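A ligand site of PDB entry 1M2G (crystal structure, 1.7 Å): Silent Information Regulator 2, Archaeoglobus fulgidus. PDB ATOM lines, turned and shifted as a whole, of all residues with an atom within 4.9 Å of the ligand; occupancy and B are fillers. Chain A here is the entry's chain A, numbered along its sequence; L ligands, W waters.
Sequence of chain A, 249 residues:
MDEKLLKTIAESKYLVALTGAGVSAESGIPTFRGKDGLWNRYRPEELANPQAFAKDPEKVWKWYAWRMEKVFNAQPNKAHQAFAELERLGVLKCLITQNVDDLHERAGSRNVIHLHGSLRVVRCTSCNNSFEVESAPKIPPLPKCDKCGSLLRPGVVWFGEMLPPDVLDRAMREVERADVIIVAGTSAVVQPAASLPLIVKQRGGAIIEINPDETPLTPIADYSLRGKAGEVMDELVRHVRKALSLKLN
The backbone NH of Ser 187 is in hydrogen-bond range of an oxygen (O8) of the ligand (3.0 Å).
O6 of the ligand is in hydrogen-bond range of OG of Ser 187 (2.6 Å).
The backbone NH (N) of Arg 33 lies within hydrogen-bond range of an oxygen (O5) of the ligand, 2.7 Å away.
The guanidinium group (NH2) of Arg 33 is in salt-bridge range of an oxygen (O6) of the ligand (2.6 Å).
An oxygen (O8) of the ligand sits at hydrogen-bond distance from the side-chain hydroxyl (OG1) of Thr 186, 2.7 Å away.
N of Phe 32 is in hydrogen-bond range of O5 of the ligand, at 2.8 Å.
A nitrogen (N1) of the ligand sits at hydrogen-bond distance from the backbone NH of Ala 229 (2.8 Å).
N of Ala 21 lies within hydrogen-bond range of O9 of the ligand, at 2.8 Å.
An oxygen (O1) of the ligand sits at hydrogen-bond distance from the side-chain amide oxygen of Asn 211 (2.8 Å).
The indole nitrogen of Trp 39 lies within hydrogen-bond range of an oxygen (O12) of the ligand (2.9 Å).
A ring nitrogen (ND1) of His 116 is in hydrogen-bond range of an oxygen (O14) of the ligand, at 2.9 Å.
The side-chain carboxylate (OE2) of Glu 26 sits at hydrogen-bond distance from a nitrogen (N3) of the ligand, at 3.1 Å.
The backbone carbonyl oxygen (O) of Gln 98 sits at hydrogen-bond distance from an oxygen (O14) of the ligand.
An oxygen (O1) of the ligand lies within hydrogen-bond range of the side-chain carboxylate (OD2) of Asp 213.
A nitrogen (N1) of the ligand sits close to the backbone carbonyl oxygen (O) of Gly 22, 3.4 Å away.
An oxygen (O3) of the ligand sits close to the backbone carbonyl oxygen (O) of Gly 185, at 3.3 Å.
Residues that only touch the ligand: Gly 20, Ala 25, Thr 31, Phe 159, Val 190, Pro 212 and Lys 228.
Hydrophobic or aromatic side chains within 4 Å of the ligand: Ala 21, Ala 25, Phe 32, Trp 39, His 116, Phe 159, Val 190, Pro 212 and Ala 229.
Of the 28 residues printed, 21 come within 4 Å of the ligand.
The backbone carbonyl oxygen (O) of Thr 186 sits at hydrogen-bond distance from the side-chain amide nitrogen (ND2) of Asn 211, at 3.1 Å.
OG1 of Thr 186 is in hydrogen-bond range of NE2 of Gln 98, at 3.0 Å.
The backbone NH (N) of Ala 229 lies within hydrogen-bond range of the side-chain carboxylate (OE2) of Glu 26 (3.4 Å).
The backbone carbonyl oxygen (O) of Gly 185 is in hydrogen-bond range of the backbone NH (N) of Ala 21, 3.3 Å away.
O of Gln 98 sits at hydrogen-bond distance from ND1 of His 116 (3.4 Å).
The backbone carbonyl oxygen of Gly 20 is in hydrogen-bond range of the side-chain amide nitrogen of Asn 99 (3.0 Å).
The backbone NH of Gly 22 is in hydrogen-bond range of the backbone carbonyl oxygen of Gly 185 (2.8 Å).
N of Gly 185 lies within hydrogen-bond range of O of Ile 210 (3.0 Å).
Water W4 bridges an oxygen (O2) of the ligand (2.7 Å) and the side-chain carboxylate (OD2) of Asp 213 (3.2 Å).
Water W2 lies within hydrogen-bond range of the side-chain amide oxygen of Asn 99 (2.7 Å), an oxygen (O9) of the ligand (2.8 Å), the backbone carbonyl oxygen of Gln 98 (3.3 Å) and the backbone NH of Ala 21 (3.4 Å).
Water W1 lies within hydrogen-bond range of the side-chain hydroxyl of Ser 187 (2.9 Å), the backbone NH of Val 190 (2.9 Å), an oxygen (O8) of the ligand (3.1 Å) and the backbone NH of Ala 188 (3.3 Å).
Water W3 lies within hydrogen-bond range of an oxygen (O1) of the ligand (3.1 Å) and the side-chain carboxylate of Asp 213 (3.4 Å).
Water W9 lies within hydrogen-bond range of O of Val 157 (2.9 Å) and O13 of the ligand (3.2 Å).
Water W8 bridges the backbone carbonyl oxygen (O) of Gln 98 and an oxygen (O14) of the ligand.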
ATOM      1  N   GLY A  20     -29.658  13.060  -8.999  1.00  0.00           N
ATOM      2  CA  GLY A  20     -28.255  13.082  -9.354  1.00  0.00           C
ATOM      3  C   GLY A  20     -27.427  13.713  -8.251  1.00  0.00           C
ATOM      4  O   GLY A  20     -27.944  14.030  -7.175  1.00  0.00           O
ATOM      5  N   ALA A  21     -26.134  13.905  -8.524  1.00  0.00           N
ATOM      6  CA  ALA A  21     -25.197  14.448  -7.538  1.00  0.00           C
ATOM      7  C   ALA A  21     -25.624  15.784  -6.912  1.00  0.00           C
ATOM      8  O   ALA A  21     -25.200  16.110  -5.800  1.00  0.00           O
ATOM      9  CB  ALA A  21     -23.822  14.602  -8.177  1.00  0.00           C
ATOM     10  N   GLY A  22     -26.430  16.543  -7.632  1.00  0.00           N
ATOM     11  CA  GLY A  22     -26.871  17.829  -7.112  1.00  0.00           C
ATOM     12  C   GLY A  22     -27.676  17.731  -5.823  1.00  0.00           C
ATOM     13  O   GLY A  22     -27.694  18.654  -5.031  1.00  0.00           O
ATOM     14  N   VAL A  23     -28.365  16.612  -5.622  1.00  0.00           N
ATOM     15  CA  VAL A  23     -29.176  16.432  -4.414  1.00  0.00           C
ATOM     16  C   VAL A  23     -28.321  16.214  -3.170  1.00  0.00           C
ATOM     17  O   VAL A  23     -28.818  16.320  -2.042  1.00  0.00           O
ATOM     18  CB  VAL A  23     -30.182  15.261  -4.608  1.00  0.00           C
ATOM     19  CG1 VAL A  23     -30.830  14.883  -3.291  1.00  0.00           C
ATOM     20  CG2 VAL A  23     -31.263  15.681  -5.614  1.00  0.00           C
ATOM     21  N   ALA A  25     -25.237  17.854  -2.879  1.00  0.00           N
ATOM     22  CA  ALA A  25     -24.328  19.000  -2.797  1.00  0.00           C
ATOM     23  C   ALA A  25     -24.457  19.733  -1.462  1.00  0.00           C
ATOM     24  O   ALA A  25     -23.461  20.160  -0.885  1.00  0.00           O
ATOM     25  CB  ALA A  25     -24.615  19.963  -3.945  1.00  0.00           C
ATOM     26  N   GLU A  26     -25.683  19.862  -0.967  1.00  0.00           N
ATOM     27  CA  GLU A  26     -25.931  20.554   0.289  1.00  0.00           C
ATOM     28  C   GLU A  26     -25.520  19.741   1.513  1.00  0.00           C
ATOM     29  O   GLU A  26     -25.740  20.160   2.656  1.00  0.00           O
ATOM     30  CB  GLU A  26     -27.398  20.973   0.362  1.00  0.00           C
ATOM     31  CG  GLU A  26     -27.741  22.018  -0.683  1.00  0.00           C
ATOM     32  CD  GLU A  26     -29.233  22.224  -0.863  1.00  0.00           C
ATOM     33  OE1 GLU A  26     -29.867  22.885  -0.010  1.00  0.00           O
ATOM     34  OE2 GLU A  26     -29.771  21.728  -1.867  1.00  0.00           O
ATOM     35  N   THR A  31     -20.300  17.975  -6.682  1.00  0.00           N
ATOM     36  CA  THR A  31     -20.942  17.278  -7.800  1.00  0.00           C
ATOM     37  C   THR A  31     -19.827  16.846  -8.739  1.00  0.00           C
ATOM     38  O   THR A  31     -18.645  16.973  -8.416  1.00  0.00           O
ATOM     39  CB  THR A  31     -21.922  18.201  -8.551  1.00  0.00           C
ATOM     40  OG1 THR A  31     -21.221  19.351  -9.048  1.00  0.00           O
ATOM     41  CG2 THR A  31     -23.042  18.656  -7.614  1.00  0.00           C
ATOM     42  N   PHE A  32     -20.182  16.309  -9.900  1.00  0.00           N
ATOM     43  CA  PHE A  32     -19.172  15.856 -10.851  1.00  0.00           C
ATOM     44  C   PHE A  32     -18.847  16.918 -11.889  1.00  0.00           C
ATOM     45  O   PHE A  32     -17.693  17.068 -12.294  1.00  0.00           O
ATOM     46  CB  PHE A  32     -19.647  14.584 -11.564  1.00  0.00           C
ATOM     47  CG  PHE A  32     -19.736  13.394 -10.662  1.00  0.00           C
ATOM     48  CD1 PHE A  32     -18.598  12.677 -10.333  1.00  0.00           C
ATOM     49  CD2 PHE A  32     -20.961  13.013 -10.124  1.00  0.00           C
ATOM     50  CE1 PHE A  32     -18.668  11.581  -9.469  1.00  0.00           C
ATOM     51  CE2 PHE A  32     -21.038  11.920  -9.267  1.00  0.00           C
ATOM     52  CZ  PHE A  32     -19.900  11.203  -8.938  1.00  0.00           C
ATOM     53  N   ARG A  33     -19.860  17.660 -12.304  1.00  0.00           N
ATOM     54  CA  ARG A  33     -19.662  18.684 -13.319  1.00  0.00           C
ATOM     55  C   ARG A  33     -19.998  20.077 -12.807  1.00  0.00           C
ATOM     56  O   ARG A  33     -20.468  20.238 -11.677  1.00  0.00           O
ATOM     57  CB  ARG A  33     -20.500  18.313 -14.547  1.00  0.00           C
ATOM     58  CG  ARG A  33     -20.189  16.895 -15.022  1.00  0.00           C
ATOM     59  CD  ARG A  33     -20.987  16.442 -16.228  1.00  0.00           C
ATOM     60  NE  ARG A  33     -20.556  15.104 -16.645  1.00  0.00           N
ATOM     61  CZ  ARG A  33     -20.849  13.979 -15.985  1.00  0.00           C
ATOM     62  NH1 ARG A  33     -20.405  12.819 -16.438  1.00  0.00           N
ATOM     63  NH2 ARG A  33     -21.589  14.025 -14.879  1.00  0.00           N
ATOM     64  N   TRP A  39     -15.049  16.077 -11.806  1.00  0.00           N
ATOM     65  CA  TRP A  39     -14.463  15.788 -13.120  1.00  0.00           C
ATOM     66  C   TRP A  39     -13.765  16.996 -13.720  1.00  0.00           C
ATOM     67  O   TRP A  39     -13.211  16.937 -14.819  1.00  0.00           O
ATOM     68  CB  TRP A  39     -15.551  15.268 -14.067  1.00  0.00           C
ATOM     69  CG  TRP A  39     -16.100  13.899 -13.731  1.00  0.00           C
ATOM     70  CD1 TRP A  39     -17.257  13.335 -14.200  1.00  0.00           C
ATOM     71  CD2 TRP A  39     -15.489  12.899 -12.882  1.00  0.00           C
ATOM     72  NE1 TRP A  39     -17.410  12.065 -13.695  1.00  0.00           N
ATOM     73  CE2 TRP A  39     -16.347  11.767 -12.893  1.00  0.00           C
ATOM     74  CE3 TRP A  39     -14.319  12.845 -12.125  1.00  0.00           C
ATOM     75  CZ2 TRP A  39     -16.059  10.600 -12.161  1.00  0.00           C
ATOM     76  CZ3 TRP A  39     -14.021  11.683 -11.403  1.00  0.00           C
ATOM     77  CH2 TRP A  39     -14.899  10.579 -11.430  1.00  0.00           C
ATOM     78  N   GLN A  98     -28.647   8.126  -9.355  1.00  0.00           N
ATOM     79  CA  GLN A  98     -27.374   7.889 -10.043  1.00  0.00           C
ATOM     80  C   GLN A  98     -26.266   8.047  -9.014  1.00  0.00           C
ATOM     81  O   GLN A  98     -25.103   7.739  -9.278  1.00  0.00           O
ATOM     82  CB  GLN A  98     -27.167   8.925 -11.140  1.00  0.00           C
ATOM     83  CG  GLN A  98     -28.192   8.854 -12.266  1.00  0.00           C
ATOM     84  CD  GLN A  98     -28.133  10.076 -13.140  1.00  0.00           C
ATOM     85  OE1 GLN A  98     -27.284  10.196 -14.026  1.00  0.00           O
ATOM     86  NE2 GLN A  98     -29.025  11.032 -12.876  1.00  0.00           N
ATOM     87  N   ASN A  99     -26.648   8.517  -7.827  1.00  0.00           N
ATOM     88  CA  ASN A  99     -25.677   8.746  -6.762  1.00  0.00           C
ATOM     89  C   ASN A  99     -25.126   7.473  -6.159  1.00  0.00           C
ATOM     90  O   ASN A  99     -25.842   6.482  -5.994  1.00  0.00           O
ATOM     91  CB  ASN A  99     -26.310   9.606  -5.666  1.00  0.00           C
ATOM     92  CG  ASN A  99     -26.688  10.979  -6.157  1.00  0.00           C
ATOM     93  OD1 ASN A  99     -26.251  11.394  -7.241  1.00  0.00           O
ATOM     94  ND2 ASN A  99     -27.493  11.703  -5.385  1.00  0.00           N
ATOM     95  N   HIS A 116     -26.016   3.467 -10.662  1.00  0.00           N
ATOM     96  CA  HIS A 116     -24.569   3.443 -10.822  1.00  0.00           C
ATOM     97  C   HIS A 116     -23.790   2.788  -9.688  1.00  0.00           C
ATOM     98  O   HIS A 116     -22.582   3.024  -9.529  1.00  0.00           O
ATOM     99  CB  HIS A 116     -24.064   4.869 -11.045  1.00  0.00           C
ATOM    100  CG  HIS A 116     -24.660   5.538 -12.243  1.00  0.00           C
ATOM    101  ND1 HIS A 116     -24.553   6.889 -12.472  1.00  0.00           N
ATOM    102  CD2 HIS A 116     -25.360   5.039 -13.297  1.00  0.00           C
ATOM    103  CE1 HIS A 116     -25.151   7.201 -13.608  1.00  0.00           C
ATOM    104  NE2 HIS A 116     -25.658   6.099 -14.126  1.00  0.00           N
ATOM    105  N   VAL A 157     -20.346   1.846 -10.927  1.00  0.00           N
ATOM    106  CA  VAL A 157     -20.255   1.670 -12.371  1.00  0.00           C
ATOM    107  C   VAL A 157     -19.368   2.736 -13.010  1.00  0.00           C
ATOM    108  O   VAL A 157     -19.615   3.934 -12.843  1.00  0.00           O
ATOM    109  CB  VAL A 157     -21.668   1.712 -13.027  1.00  0.00           C
ATOM    110  CG1 VAL A 157     -21.549   1.507 -14.543  1.00  0.00           C
ATOM    111  CG2 VAL A 157     -22.553   0.638 -12.423  1.00  0.00           C
ATOM    112  N   PHE A 159     -17.221   4.475 -16.439  1.00  0.00           N
ATOM    113  CA  PHE A 159     -17.489   4.791 -17.837  1.00  0.00           C
ATOM    114  C   PHE A 159     -17.185   3.597 -18.743  1.00  0.00           C
ATOM    115  O   PHE A 159     -16.141   2.952 -18.592  1.00  0.00           O
ATOM    116  CB  PHE A 159     -16.660   5.991 -18.295  1.00  0.00           C
ATOM    117  CG  PHE A 159     -17.139   7.311 -17.753  1.00  0.00           C
ATOM    118  CD1 PHE A 159     -16.640   7.813 -16.548  1.00  0.00           C
ATOM    119  CD2 PHE A 159     -18.115   8.034 -18.430  1.00  0.00           C
ATOM    120  CE1 PHE A 159     -17.111   9.022 -16.034  1.00  0.00           C
ATOM    121  CE2 PHE A 159     -18.594   9.245 -17.922  1.00  0.00           C
ATOM    122  CZ  PHE A 159     -18.082   9.741 -16.718  1.00  0.00           C
ATOM    123  N   GLY A 185     -31.301  17.540  -9.345  1.00  0.00           N
ATOM    124  CA  GLY A 185     -29.851  17.499  -9.221  1.00  0.00           C
ATOM    125  C   GLY A 185     -29.056  16.705 -10.234  1.00  0.00           C
ATOM    126  O   GLY A 185     -27.992  16.193  -9.897  1.00  0.00           O
ATOM    127  N   THR A 186     -29.530  16.601 -11.467  1.00  0.00           N
ATOM    128  CA  THR A 186     -28.772  15.874 -12.463  1.00  0.00           C
ATOM    129  C   THR A 186     -28.625  16.724 -13.718  1.00  0.00           C
ATOM    130  O   THR A 186     -29.538  17.445 -14.115  1.00  0.00           O
ATOM    131  CB  THR A 186     -29.419  14.505 -12.799  1.00  0.00           C
ATOM    132  OG1 THR A 186     -28.656  13.859 -13.823  1.00  0.00           O
ATOM    133  CG2 THR A 186     -30.867  14.676 -13.254  1.00  0.00           C
ATOM    134  N   SER A 187     -27.441  16.637 -14.323  1.00  0.00           N
ATOM    135  CA  SER A 187     -27.118  17.405 -15.525  1.00  0.00           C
ATOM    136  C   SER A 187     -27.741  16.866 -16.800  1.00  0.00           C
ATOM    137  O   SER A 187     -27.637  17.486 -17.863  1.00  0.00           O
ATOM    138  CB  SER A 187     -25.605  17.499 -15.675  1.00  0.00           C
ATOM    139  OG  SER A 187     -25.022  16.221 -15.754  1.00  0.00           O
ATOM    140  N   ALA A 188     -28.376  15.695 -16.721  1.00  0.00           N
ATOM    141  CA  ALA A 188     -29.059  15.079 -17.861  1.00  0.00           C
ATOM    142  C   ALA A 188     -28.200  14.858 -19.107  1.00  0.00           C
ATOM    143  O   ALA A 188     -28.673  15.070 -20.230  1.00  0.00           O
ATOM    144  CB  ALA A 188     -30.285  15.897 -18.229  1.00  0.00           C
ATOM    145  N   VAL A 190     -25.458  12.111 -18.882  1.00  0.00           N
ATOM    146  CA  VAL A 190     -25.003  10.724 -18.804  1.00  0.00           C
ATOM    147  C   VAL A 190     -26.100   9.706 -19.111  1.00  0.00           C
ATOM    148  O   VAL A 190     -27.176   9.723 -18.496  1.00  0.00           O
ATOM    149  CB  VAL A 190     -24.417  10.417 -17.408  1.00  0.00           C
ATOM    150  CG1 VAL A 190     -24.093   8.932 -17.290  1.00  0.00           C
ATOM    151  CG2 VAL A 190     -23.156  11.234 -17.209  1.00  0.00           C
ATOM    152  N   ILE A 210     -35.838  19.917 -11.028  1.00  0.00           N
ATOM    153  CA  ILE A 210     -35.352  20.769  -9.948  1.00  0.00           C
ATOM    154  C   ILE A 210     -33.837  20.870 -10.114  1.00  0.00           C
ATOM    155  O   ILE A 210     -33.107  19.891  -9.898  1.00  0.00           O
ATOM    156  CB  ILE A 210     -35.664  20.181  -8.565  1.00  0.00           C
ATOM    157  CG1 ILE A 210     -37.177  20.034  -8.400  1.00  0.00           C
ATOM    158  CG2 ILE A 210     -35.110  21.092  -7.482  1.00  0.00           C
ATOM    159  CD1 ILE A 210     -37.582  19.345  -7.112  1.00  0.00           C
ATOM    160  N   ASN A 211     -33.363  22.054 -10.484  1.00  0.00           N
ATOM    161  CA  ASN A 211     -31.942  22.249 -10.731  1.00  0.00           C
ATOM    162  C   ASN A 211     -31.658  23.742 -10.855  1.00  0.00           C
ATOM    163  O   ASN A 211     -32.419  24.466 -11.483  1.00  0.00           O
ATOM    164  CB  ASN A 211     -31.586  21.547 -12.052  1.00  0.00           C
ATOM    165  CG  ASN A 211     -30.099  21.327 -12.208  1.00  0.00           C
ATOM    166  OD1 ASN A 211     -29.292  22.253 -12.064  1.00  0.00           O
ATOM    167  ND2 ASN A 211     -29.720  20.098 -12.548  1.00  0.00           N
ATOM    168  N   PRO A 212     -30.548  24.222 -10.252  1.00  0.00           N
ATOM    169  CA  PRO A 212     -30.219  25.643 -10.356  1.00  0.00           C
ATOM    170  C   PRO A 212     -29.824  26.049 -11.780  1.00  0.00           C
ATOM    171  O   PRO A 212     -29.850  27.221 -12.130  1.00  0.00           O
ATOM    172  CB  PRO A 212     -29.070  25.809  -9.356  1.00  0.00           C
ATOM    173  CG  PRO A 212     -28.455  24.449  -9.326  1.00  0.00           C
ATOM    174  CD  PRO A 212     -29.645  23.542  -9.326  1.00  0.00           C
ATOM    175  N   ASP A 213     -29.455  25.060 -12.588  1.00  0.00           N
ATOM    176  CA  ASP A 213     -29.082  25.303 -13.977  1.00  0.00           C
ATOM    177  C   ASP A 213     -30.102  24.676 -14.910  1.00  0.00           C
ATOM    178  O   ASP A 213     -30.884  23.811 -14.510  1.00  0.00           O
ATOM    179  CB  ASP A 213     -27.718  24.671 -14.320  1.00  0.00           C
ATOM    180  CG  ASP A 213     -26.553  25.331 -13.600  1.00  0.00           C
ATOM    181  OD1 ASP A 213     -26.696  26.478 -13.135  1.00  0.00           O
ATOM    182  OD2 ASP A 213     -25.487  24.695 -13.519  1.00  0.00           O
ATOM    183  N   THR A 215     -30.803  22.362 -18.205  1.00  0.00           N
ATOM    184  CA  THR A 215     -30.113  21.185 -18.725  1.00  0.00           C
ATOM    185  C   THR A 215     -30.776  20.761 -20.027  1.00  0.00           C
ATOM    186  O   THR A 215     -31.775  21.357 -20.458  1.00  0.00           O
ATOM    187  CB  THR A 215     -30.226  20.000 -17.748  1.00  0.00           C
ATOM    188  OG1 THR A 215     -31.530  19.425 -17.856  1.00  0.00           O
ATOM    189  CG2 THR A 215     -29.985  20.458 -16.314  1.00  0.00           C
ATOM    190  N   GLY A 227     -33.586  26.254  -8.506  1.00  0.00           N
ATOM    191  CA  GLY A 227     -33.203  26.443  -7.130  1.00  0.00           C
ATOM    192  C   GLY A 227     -32.547  25.185  -6.594  1.00  0.00           C
ATOM    193  O   GLY A 227     -32.507  24.164  -7.273  1.00  0.00           O
ATOM    194  N   LYS A 228     -32.008  25.278  -5.375  1.00  0.00           N
ATOM    195  CA  LYS A 228     -31.353  24.153  -4.751  1.00  0.00           C
ATOM    196  C   LYS A 228     -32.401  23.125  -4.333  1.00  0.00           C
ATOM    197  O   LYS A 228     -33.512  23.491  -3.941  1.00  0.00           O
ATOM    198  CB  LYS A 228     -30.559  24.613  -3.523  1.00  0.00           C
ATOM    199  CG  LYS A 228     -29.409  25.546  -3.854  1.00  0.00           C
ATOM    200  CD  LYS A 228     -28.607  25.872  -2.599  1.00  0.00           C
ATOM    201  CE  LYS A 228     -27.405  26.735  -2.933  1.00  0.00           C
ATOM    202  NZ  LYS A 228     -26.559  27.029  -1.738  1.00  0.00           N
ATOM    203  N   ALA A 229     -32.052  21.851  -4.424  1.00  0.00           N
ATOM    204  CA  ALA A 229     -32.990  20.781  -4.066  1.00  0.00           C
ATOM    205  C   ALA A 229     -33.440  20.812  -2.615  1.00  0.00           C
ATOM    206  O   ALA A 229     -34.597  20.505  -2.315  1.00  0.00           O
ATOM    207  CB  ALA A 229     -32.355  19.428  -4.378  1.00  0.00           C
HETATM  208  N1  LIG L   1     -29.689  21.256  -5.770  1.00  0.00           N
HETATM  209  C1  LIG L   1     -30.090  20.663  -6.974  1.00  0.00           C
HETATM  210  N2  LIG L   1     -29.182  20.551  -8.027  1.00  0.00           N
HETATM  211  C2  LIG L   1     -27.879  21.035  -7.870  1.00  0.00           C
HETATM  212  C3  LIG L   1     -27.473  21.623  -6.673  1.00  0.00           C
HETATM  213  C4  LIG L   1     -28.395  21.750  -5.584  1.00  0.00           C
HETATM  214  N3  LIG L   1     -28.039  22.303  -4.403  1.00  0.00           N
HETATM  215  N4  LIG L   1     -26.214  21.988  -6.794  1.00  0.00           N
HETATM  216  C5  LIG L   1     -25.827  21.622  -8.062  1.00  0.00           C
HETATM  217  N5  LIG L   1     -26.861  20.993  -8.826  1.00  0.00           N
HETATM  218  C6  LIG L   1     -26.972  20.426 -10.118  1.00  0.00           C
HETATM  219  C7  LIG L   1     -26.110  21.012 -11.106  1.00  0.00           C
HETATM  220  O1  LIG L   1     -26.510  22.178 -11.620  1.00  0.00           O
HETATM  221  C8  LIG L   1     -25.938  19.954 -12.036  1.00  0.00           C
HETATM  222  O2  LIG L   1     -26.770  20.046 -13.083  1.00  0.00           O
HETATM  223  O3  LIG L   1     -26.565  19.156 -10.072  1.00  0.00           O
HETATM  224  C9  LIG L   1     -26.238  18.743 -11.317  1.00  0.00           C
HETATM  225  C10 LIG L   1     -25.173  17.755 -11.204  1.00  0.00           C
HETATM  226  O4  LIG L   1     -24.781  17.309 -12.410  1.00  0.00           O
HETATM  227  P1  LIG L   1     -23.584  16.182 -12.394  1.00  0.00           P
HETATM  228  O5  LIG L   1     -22.336  16.695 -11.598  1.00  0.00           O
HETATM  229  O6  LIG L   1     -23.245  15.811 -13.886  1.00  0.00           O
HETATM  230  O7  LIG L   1     -24.146  14.902 -11.571  1.00  0.00           O
HETATM  231  P2  LIG L   1     -24.986  13.702 -12.268  1.00  0.00           P
HETATM  232  O8  LIG L   1     -26.056  14.184 -13.328  1.00  0.00           O
HETATM  233  O9  LIG L   1     -25.677  12.909 -11.091  1.00  0.00           O
HETATM  234  O10 LIG L   1     -23.853  12.767 -12.952  1.00  0.00           O
HETATM  235  C11 LIG L   1     -24.251  11.678 -13.589  1.00  0.00           C
HETATM  236  O11 LIG L   1     -22.013  11.079 -14.029  1.00  0.00           O
HETATM  237  O12 LIG L   1     -19.845  10.541 -13.927  1.00  0.00           O
HETATM  238  C12 LIG L   1     -21.032  10.935 -13.210  1.00  0.00           C
HETATM  239  O13 LIG L   1     -21.459   8.418 -12.671  1.00  0.00           O
HETATM  240  C13 LIG L   1     -21.466   9.712 -12.421  1.00  0.00           C
HETATM  241  O14 LIG L   1     -23.623   9.471 -11.531  1.00  0.00           O
HETATM  242  C14 LIG L   1     -22.785  10.259 -12.215  1.00  0.00           C
HETATM  243  C15 LIG L   1     -23.179  10.677 -13.518  1.00  0.00           C
HETATM  244  O   HOH W   1     -25.943  13.515 -16.360  1.00  0.00           O
HETATM  245  O   HOH W   2     -24.639  10.997  -9.388  1.00  0.00           O
HETATM  246  O   HOH W   3     -25.303  24.645 -10.151  1.00  0.00           O
HETATM  247  O   HOH W   4     -25.792  21.809 -14.824  1.00  0.00           O
HETATM  248  O   HOH W   5     -22.952  21.249 -12.400  1.00  0.00           O
HETATM  249  O   HOH W   6     -23.804  23.110  -5.782  1.00  0.00           O
HETATM  250  O   HOH W   7     -22.878  21.561  -9.780  1.00  0.00           O
HETATM  251  O   HOH W   8     -22.497   8.770  -8.575  1.00  0.00           O
HETATM  252  O   HOH W   9     -20.224   5.999 -10.961  1.00  0.00           O
HETATM  253  O   HOH W  10     -25.632  23.660  -3.608  1.00  0.00           O
